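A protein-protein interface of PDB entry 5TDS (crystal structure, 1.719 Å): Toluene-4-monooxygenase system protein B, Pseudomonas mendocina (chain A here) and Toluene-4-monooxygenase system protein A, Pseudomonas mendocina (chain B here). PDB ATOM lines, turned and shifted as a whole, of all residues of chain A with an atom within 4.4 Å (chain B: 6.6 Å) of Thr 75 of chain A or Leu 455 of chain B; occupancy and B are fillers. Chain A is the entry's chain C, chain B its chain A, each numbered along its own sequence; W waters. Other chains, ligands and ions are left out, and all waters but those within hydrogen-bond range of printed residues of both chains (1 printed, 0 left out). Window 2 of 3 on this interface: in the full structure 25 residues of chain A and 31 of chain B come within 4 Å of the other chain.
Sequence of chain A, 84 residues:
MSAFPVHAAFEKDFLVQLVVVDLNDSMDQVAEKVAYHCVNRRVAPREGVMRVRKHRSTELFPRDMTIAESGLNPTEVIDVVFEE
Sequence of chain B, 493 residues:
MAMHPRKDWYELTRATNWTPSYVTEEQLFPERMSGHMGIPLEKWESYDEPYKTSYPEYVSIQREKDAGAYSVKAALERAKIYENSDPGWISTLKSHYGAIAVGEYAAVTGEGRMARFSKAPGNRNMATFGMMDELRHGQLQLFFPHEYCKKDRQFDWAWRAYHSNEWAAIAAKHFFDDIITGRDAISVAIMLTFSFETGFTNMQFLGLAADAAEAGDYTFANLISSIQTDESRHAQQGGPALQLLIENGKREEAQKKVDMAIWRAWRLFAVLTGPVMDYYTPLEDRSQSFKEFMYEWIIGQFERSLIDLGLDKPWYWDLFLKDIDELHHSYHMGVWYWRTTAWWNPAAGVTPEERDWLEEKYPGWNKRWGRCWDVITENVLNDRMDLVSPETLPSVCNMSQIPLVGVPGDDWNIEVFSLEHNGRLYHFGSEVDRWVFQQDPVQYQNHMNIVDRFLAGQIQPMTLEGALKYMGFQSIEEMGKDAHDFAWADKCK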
ATOM      1  N   PRO A   5     -17.811   5.594   1.332  1.00  0.00           N
ATOM      2  CA  PRO A   5     -16.650   4.796   0.929  1.00  0.00           C
ATOM      3  C   PRO A   5     -15.684   4.549   2.080  1.00  0.00           C
ATOM      4  O   PRO A   5     -15.379   5.468   2.845  1.00  0.00           O
ATOM      5  CB  PRO A   5     -15.986   5.656  -0.153  1.00  0.00           C
ATOM      6  CG  PRO A   5     -16.394   7.060   0.186  1.00  0.00           C
ATOM      7  CD  PRO A   5     -17.795   6.947   0.744  1.00  0.00           C
ATOM      8  N   HIS A   7     -11.808   2.299   2.887  1.00  0.00           N
ATOM      9  CA  HIS A   7     -10.744   1.446   2.382  1.00  0.00           C
ATOM     10  C   HIS A   7     -10.542   0.365   3.415  1.00  0.00           C
ATOM     11  O   HIS A   7     -10.236   0.667   4.564  1.00  0.00           O
ATOM     12  CB  HIS A   7      -9.472   2.238   2.146  1.00  0.00           C
ATOM     13  CG  HIS A   7      -9.619   3.290   1.100  1.00  0.00           C
ATOM     14  ND1 HIS A   7      -9.722   2.990  -0.242  1.00  0.00           N
ATOM     15  CD2 HIS A   7      -9.714   4.636   1.195  1.00  0.00           C
ATOM     16  CE1 HIS A   7      -9.857   4.109  -0.931  1.00  0.00           C
ATOM     17  NE2 HIS A   7      -9.859   5.124  -0.082  1.00  0.00           N
ATOM     18  N   LEU A  18     -11.234  -0.738  -1.995  1.00  0.00           N
ATOM     19  CA  LEU A  18     -12.350   0.188  -1.872  1.00  0.00           C
ATOM     20  C   LEU A  18     -13.629  -0.609  -1.681  1.00  0.00           C
ATOM     21  O   LEU A  18     -13.947  -1.479  -2.486  1.00  0.00           O
ATOM     22  CB  LEU A  18     -12.455   1.086  -3.106  1.00  0.00           C
ATOM     23  CG  LEU A  18     -13.726   1.941  -3.141  1.00  0.00           C
ATOM     24  CD1 LEU A  18     -13.732   2.918  -1.978  1.00  0.00           C
ATOM     25  CD2 LEU A  18     -13.846   2.673  -4.467  1.00  0.00           C
ATOM     26  N   ASN A  73     -14.824   8.696   9.224  1.00  0.00           N
ATOM     27  CA  ASN A  73     -15.067   9.598   8.114  1.00  0.00           C
ATOM     28  C   ASN A  73     -14.880   8.876   6.798  1.00  0.00           C
ATOM     29  O   ASN A  73     -14.130   7.906   6.732  1.00  0.00           O
ATOM     30  CB  ASN A  73     -14.137  10.802   8.194  1.00  0.00           C
ATOM     31  CG  ASN A  73     -14.315  11.576   9.477  1.00  0.00           C
ATOM     32  OD1 ASN A  73     -15.385  12.113   9.737  1.00  0.00           O
ATOM     33  ND2 ASN A  73     -13.273  11.623  10.293  1.00  0.00           N
ATOM     34  N   PRO A  74     -15.564   9.344   5.743  1.00  0.00           N
ATOM     35  CA  PRO A  74     -15.429   8.756   4.408  1.00  0.00           C
ATOM     36  C   PRO A  74     -13.973   8.645   3.959  1.00  0.00           C
ATOM     37  O   PRO A  74     -13.189   9.570   4.172  1.00  0.00           O
ATOM     38  CB  PRO A  74     -16.197   9.734   3.517  1.00  0.00           C
ATOM     39  CG  PRO A  74     -17.210  10.316   4.420  1.00  0.00           C
ATOM     40  CD  PRO A  74     -16.528  10.456   5.752  1.00  0.00           C
ATOM     41  N   THR A  75     -13.650   7.506   3.353  1.00  0.00           N
ATOM     42  CA  THR A  75     -12.323   7.169   2.817  1.00  0.00           C
ATOM     43  C   THR A  75     -11.262   6.864   3.886  1.00  0.00           C
ATOM     44  O   THR A  75     -10.092   6.673   3.562  1.00  0.00           O
ATOM     45  CB  THR A  75     -11.771   8.283   1.864  1.00  0.00           C
ATOM     46  OG1 THR A  75     -11.323   9.422   2.606  1.00  0.00           O
ATOM     47  CG2 THR A  75     -12.832   8.712   0.858  1.00  0.00           C
ATOM     48  N   GLU A  76     -11.646   6.780   5.151  1.00  0.00           N
ATOM     49  CA  GLU A  76     -10.675   6.333   6.144  1.00  0.00           C
ATOM     50  C   GLU A  76     -10.455   4.831   5.977  1.00  0.00           C
ATOM     51  O   GLU A  76     -11.233   4.148   5.305  1.00  0.00           O
ATOM     52  CB  GLU A  76     -11.125   6.700   7.567  1.00  0.00           C
ATOM     53  CG  GLU A  76     -11.089   8.207   7.784  1.00  0.00           C
ATOM     54  CD  GLU A  76     -11.318   8.633   9.227  1.00  0.00           C
ATOM     55  OE1 GLU A  76     -11.918   7.860  10.005  1.00  0.00           O
ATOM     56  OE2 GLU A  76     -10.896   9.756   9.575  1.00  0.00           O
ATOM     57  N   VAL A  77      -9.371   4.326   6.552  1.00  0.00           N
ATOM     58  CA  VAL A  77      -9.012   2.923   6.394  1.00  0.00           C
ATOM     59  C   VAL A  77      -9.478   2.111   7.600  1.00  0.00           C
ATOM     60  O   VAL A  77      -9.286   2.519   8.743  1.00  0.00           O
ATOM     61  CB  VAL A  77      -7.494   2.757   6.211  1.00  0.00           C
ATOM     62  CG1 VAL A  77      -7.135   1.294   6.011  1.00  0.00           C
ATOM     63  CG2 VAL A  77      -7.016   3.594   5.031  1.00  0.00           C
ATOM     64  N   LEU B 425      -7.516  13.873   2.941  1.00  0.00           N
ATOM     65  CA  LEU B 425      -6.917  12.642   3.445  1.00  0.00           C
ATOM     66  C   LEU B 425      -6.250  11.853   2.319  1.00  0.00           C
ATOM     67  O   LEU B 425      -6.926  11.383   1.393  1.00  0.00           O
ATOM     68  CB  LEU B 425      -7.975  11.773   4.138  1.00  0.00           C
ATOM     69  CG  LEU B 425      -7.461  10.460   4.748  1.00  0.00           C
ATOM     70  CD1 LEU B 425      -6.339  10.707   5.762  1.00  0.00           C
ATOM     71  CD2 LEU B 425      -8.594   9.668   5.385  1.00  0.00           C
ATOM     72  N   HIS B 427      -3.547   8.618   1.219  1.00  0.00           N
ATOM     73  CA  HIS B 427      -3.086   7.303   1.669  1.00  0.00           C
ATOM     74  C   HIS B 427      -1.871   6.852   0.891  1.00  0.00           C
ATOM     75  O   HIS B 427      -1.851   6.973  -0.327  1.00  0.00           O
ATOM     76  CB  HIS B 427      -4.188   6.266   1.522  1.00  0.00           C
ATOM     77  CG  HIS B 427      -5.423   6.591   2.299  1.00  0.00           C
ATOM     78  ND1 HIS B 427      -5.431   6.680   3.673  1.00  0.00           N
ATOM     79  CD2 HIS B 427      -6.691   6.839   1.896  1.00  0.00           C
ATOM     80  CE1 HIS B 427      -6.652   6.977   4.086  1.00  0.00           C
ATOM     81  NE2 HIS B 427      -7.436   7.076   3.028  1.00  0.00           N
ATOM     82  N   MET B 448      -5.105  13.646  -8.344  1.00  0.00           N
ATOM     83  CA  MET B 448      -6.127  12.653  -8.034  1.00  0.00           C
ATOM     84  C   MET B 448      -5.752  11.300  -8.611  1.00  0.00           C
ATOM     85  O   MET B 448      -5.575  11.181  -9.822  1.00  0.00           O
ATOM     86  CB  MET B 448      -7.480  13.089  -8.602  1.00  0.00           C
ATOM     87  CG  MET B 448      -7.962  14.424  -8.088  1.00  0.00           C
ATOM     88  SD  MET B 448      -8.702  14.249  -6.459  1.00  0.00           S
ATOM     89  CE  MET B 448     -10.283  13.520  -6.885  1.00  0.00           C
ATOM     90  N   ILE B 450      -6.607   7.237  -9.520  1.00  0.00           N
ATOM     91  CA  ILE B 450      -7.748   6.754 -10.274  1.00  0.00           C
ATOM     92  C   ILE B 450      -8.928   6.430  -9.351  1.00  0.00           C
ATOM     93  O   ILE B 450     -10.078   6.635  -9.735  1.00  0.00           O
ATOM     94  CB  ILE B 450      -7.345   5.535 -11.133  1.00  0.00           C
ATOM     95  CG1 ILE B 450      -8.477   5.134 -12.082  1.00  0.00           C
ATOM     96  CG2 ILE B 450      -6.861   4.390 -10.253  1.00  0.00           C
ATOM     97  CD1 ILE B 450      -8.019   4.177 -13.171  1.00  0.00           C
ATOM     98  N   VAL B 451      -8.656   5.968  -8.130  1.00  0.00           N
ATOM     99  CA  VAL B 451      -9.739   5.732  -7.167  1.00  0.00           C
ATOM    100  C   VAL B 451     -10.337   7.047  -6.657  1.00  0.00           C
ATOM    101  O   VAL B 451     -11.552   7.143  -6.451  1.00  0.00           O
ATOM    102  CB  VAL B 451      -9.260   4.885  -5.960  1.00  0.00           C
ATOM    103  CG1 VAL B 451     -10.398   4.676  -4.981  1.00  0.00           C
ATOM    104  CG2 VAL B 451      -8.724   3.535  -6.429  1.00  0.00           C
ATOM    105  N   ASP B 452      -9.497   8.062  -6.446  1.00  0.00           N
ATOM    106  CA  ASP B 452     -10.010   9.388  -6.102  1.00  0.00           C
ATOM    107  C   ASP B 452     -10.989   9.883  -7.175  1.00  0.00           C
ATOM    108  O   ASP B 452     -12.017  10.485  -6.860  1.00  0.00           O
ATOM    109  CB  ASP B 452      -8.878  10.411  -5.943  1.00  0.00           C
ATOM    110  CG  ASP B 452      -7.885  10.040  -4.844  1.00  0.00           C
ATOM    111  OD1 ASP B 452      -8.300   9.492  -3.794  1.00  0.00           O
ATOM    112  OD2 ASP B 452      -6.681  10.303  -5.035  1.00  0.00           O
ATOM    113  N   ARG B 453     -10.648   9.651  -8.440  1.00  0.00           N
ATOM    114  CA  ARG B 453     -11.495  10.082  -9.549  1.00  0.00           C
ATOM    115  C   ARG B 453     -12.783   9.285  -9.576  1.00  0.00           C
ATOM    116  O   ARG B 453     -13.858   9.821  -9.836  1.00  0.00           O
ATOM    117  CB  ARG B 453     -10.755   9.938 -10.881  1.00  0.00           C
ATOM    118  CG  ARG B 453      -9.424  10.677 -10.888  1.00  0.00           C
ATOM    119  CD  ARG B 453      -8.660  10.453 -12.185  1.00  0.00           C
ATOM    120  NE  ARG B 453      -7.245  10.755 -11.996  1.00  0.00           N
ATOM    121  CZ  ARG B 453      -6.326  10.688 -12.954  1.00  0.00           C
ATOM    122  NH1 ARG B 453      -6.670  10.334 -14.189  1.00  0.00           N
ATOM    123  NH2 ARG B 453      -5.063  10.975 -12.674  1.00  0.00           N
ATOM    124  N   PHE B 454     -12.654   7.992  -9.309  1.00  0.00           N
ATOM    125  CA  PHE B 454     -13.787   7.084  -9.161  1.00  0.00           C
ATOM    126  C   PHE B 454     -14.769   7.593  -8.100  1.00  0.00           C
ATOM    127  O   PHE B 454     -15.975   7.670  -8.330  1.00  0.00           O
ATOM    128  CB  PHE B 454     -13.258   5.697  -8.787  1.00  0.00           C
ATOM    129  CG  PHE B 454     -14.273   4.597  -8.878  1.00  0.00           C
ATOM    130  CD1 PHE B 454     -14.671   4.103 -10.110  1.00  0.00           C
ATOM    131  CD2 PHE B 454     -14.786   4.017  -7.727  1.00  0.00           C
ATOM    132  CE1 PHE B 454     -15.587   3.070 -10.192  1.00  0.00           C
ATOM    133  CE2 PHE B 454     -15.701   2.980  -7.802  1.00  0.00           C
ATOM    134  CZ  PHE B 454     -16.100   2.503  -9.033  1.00  0.00           C
ATOM    135  N   LEU B 455     -14.249   7.959  -6.937  1.00  0.00           N
ATOM    136  CA  LEU B 455     -15.114   8.447  -5.865  1.00  0.00           C
ATOM    137  C   LEU B 455     -15.675   9.843  -6.145  1.00  0.00           C
ATOM    138  O   LEU B 455     -16.758  10.190  -5.659  1.00  0.00           O
ATOM    139  CB  LEU B 455     -14.350   8.439  -4.542  1.00  0.00           C
ATOM    140  CG  LEU B 455     -13.984   7.029  -4.056  1.00  0.00           C
ATOM    141  CD1 LEU B 455     -13.175   7.091  -2.774  1.00  0.00           C
ATOM    142  CD2 LEU B 455     -15.243   6.176  -3.851  1.00  0.00           C
ATOM    143  N   ALA B 456     -14.951  10.638  -6.927  1.00  0.00           N
ATOM    144  CA  ALA B 456     -15.369  12.008  -7.226  1.00  0.00           C
ATOM    145  C   ALA B 456     -16.423  12.095  -8.334  1.00  0.00           C
ATOM    146  O   ALA B 456     -16.964  13.171  -8.595  1.00  0.00           O
ATOM    147  CB  ALA B 456     -14.157  12.853  -7.597  1.00  0.00           C
ATOM    148  N   GLY B 457     -16.715  10.979  -8.990  1.00  0.00           N
ATOM    149  CA  GLY B 457     -17.750  10.964 -10.010  1.00  0.00           C
ATOM    150  C   GLY B 457     -17.286  11.066 -11.456  1.00  0.00           C
ATOM    151  O   GLY B 457     -18.108  11.193 -12.359  1.00  0.00           O
ATOM    152  N   GLN B 458     -15.979  10.982 -11.685  1.00  0.00           N
ATOM    153  CA  GLN B 458     -15.429  11.155 -13.032  1.00  0.00           C
ATOM    154  C   GLN B 458     -15.550   9.891 -13.884  1.00  0.00           C
ATOM    155  O   GLN B 458     -15.378   9.935 -15.106  1.00  0.00           O
ATOM    156  CB  GLN B 458     -13.953  11.582 -12.955  1.00  0.00           C
ATOM    157  CG  GLN B 458     -13.717  12.874 -12.177  1.00  0.00           C
ATOM    158  CD  GLN B 458     -12.240  13.225 -12.023  1.00  0.00           C
ATOM    159  OE1 GLN B 458     -11.411  12.892 -12.878  1.00  0.00           O
ATOM    160  NE2 GLN B 458     -11.902  13.903 -10.922  1.00  0.00           N
ATOM    161  N   ILE B 459     -15.824   8.764 -13.233  1.00  0.00           N
ATOM    162  CA  ILE B 459     -15.848   7.478 -13.923  1.00  0.00           C
ATOM    163  C   ILE B 459     -17.241   6.899 -13.902  1.00  0.00           C
ATOM    164  O   ILE B 459     -17.731   6.501 -12.846  1.00  0.00           O
ATOM    165  CB  ILE B 459     -14.871   6.471 -13.287  1.00  0.00           C
ATOM    166  CG1 ILE B 459     -13.449   7.034 -13.326  1.00  0.00           C
ATOM    167  CG2 ILE B 459     -14.961   5.131 -13.993  1.00  0.00           C
ATOM    168  CD1 ILE B 459     -12.395   6.115 -12.735  1.00  0.00           C
ATOM    169  N   MET B 462     -20.167   3.945 -12.238  1.00  0.00           N
ATOM    170  CA  MET B 462     -19.242   3.814 -11.128  1.00  0.00           C
ATOM    171  C   MET B 462     -19.117   2.338 -10.748  1.00  0.00           C
ATOM    172  O   MET B 462     -19.576   1.892  -9.692  1.00  0.00           O
ATOM    173  CB  MET B 462     -19.704   4.667  -9.949  1.00  0.00           C
ATOM    174  CG  MET B 462     -18.612   4.984  -8.955  1.00  0.00           C
ATOM    175  SD  MET B 462     -19.270   5.873  -7.541  1.00  0.00           S
ATOM    176  CE  MET B 462     -17.902   5.735  -6.398  1.00  0.00           C
HETATM  177  O   HOH W   1      -8.928   9.654   1.440  1.00  0.00           O
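N of His 7 of chain A is in hydrogen-bond range of O of Glu 76 of chain A (3.1 Å).
The backbone carbonyl oxygen (O) of Pro 5 of chain A sits at hydrogen-bond distance from the backbone NH (N) of Thr 75 of chain A.
ND2 of Asn 73 of chain A sits at hydrogen-bond distance from OE2 of Glu 76 of chain A.
Hydrophobic or aromatic side chains of chain B within 4 Å of the printed part of chain A: Leu 425, His 427, Phe 454 and Leu 455.
Printed residues of chain A that touch a printed residue of chain B: Pro 5, His 7, Leu 18, Thr 75, Glu 76 and Val 77.
Hydrophobic or aromatic side chains of chain A within 4 Å of the printed part of chain B: Pro 5, His 7, Leu 18 and Val 77.
Among the printed residues, 9 pairs touch across the chains.
Water W1 lies within hydrogen-bond range of the backbone carbonyl oxygen (O) of Leu 425 of chain B (2.6 Å), the side-chain hydroxyl (OG1) of Thr 75 of chain A (2.7 Å) and a ring nitrogen (NE2) of His 427 of chain B (3.4 Å).
Among the printed residues, merely in contact across the chains: Val 77 of chain A with His 427 of chain B, Leu 18 of chain A with Phe 454 of chain B, Glu 76 of chain A with Leu 425 of chain B, His 7 of chain A with His 427 of chain B, Pro 5 of chain A with Leu 455 of chain B, Thr 75 of chain A with Leu 425 of chain B, Leu 18 of chain A with Leu 455 of chain B and Thr 75 of chain A with Leu 455 of chain B.
NE2 of His 427 of chain B sits at hydrogen-bond distance from O of Thr 75 of chain A.
Printed residues of chain B within 4 Å of Thr 75 of chain A: Leu 425, His 427 and Leu 455.
Printed residues of chain A within 4 Å of Leu 455 of chain B: Pro 5, Leu 18 and Thr 75.
Of the printed residues of chain A, His 427 of chain B touches His 7, Thr 75 and Val 77.
Of the printed residues of chain B, Pro 5 of chain A touches Leu 455.
Of the printed residues of chain A, Leu 425 of chain B touches Thr 75 (3.8 Å) and Glu 76 (3.8 Å).
Printed residues of chain B within 4 Å of Val 77 of chain A: His 427.
Printed residues of chain A within 4 Å of Phe 454 of chain B: Leu 18 (3.6 Å).
Pro 74 of chain A touches none of the printed residues of chain B.
Ile 450 of chain B touches none of the printed residues of chain A.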
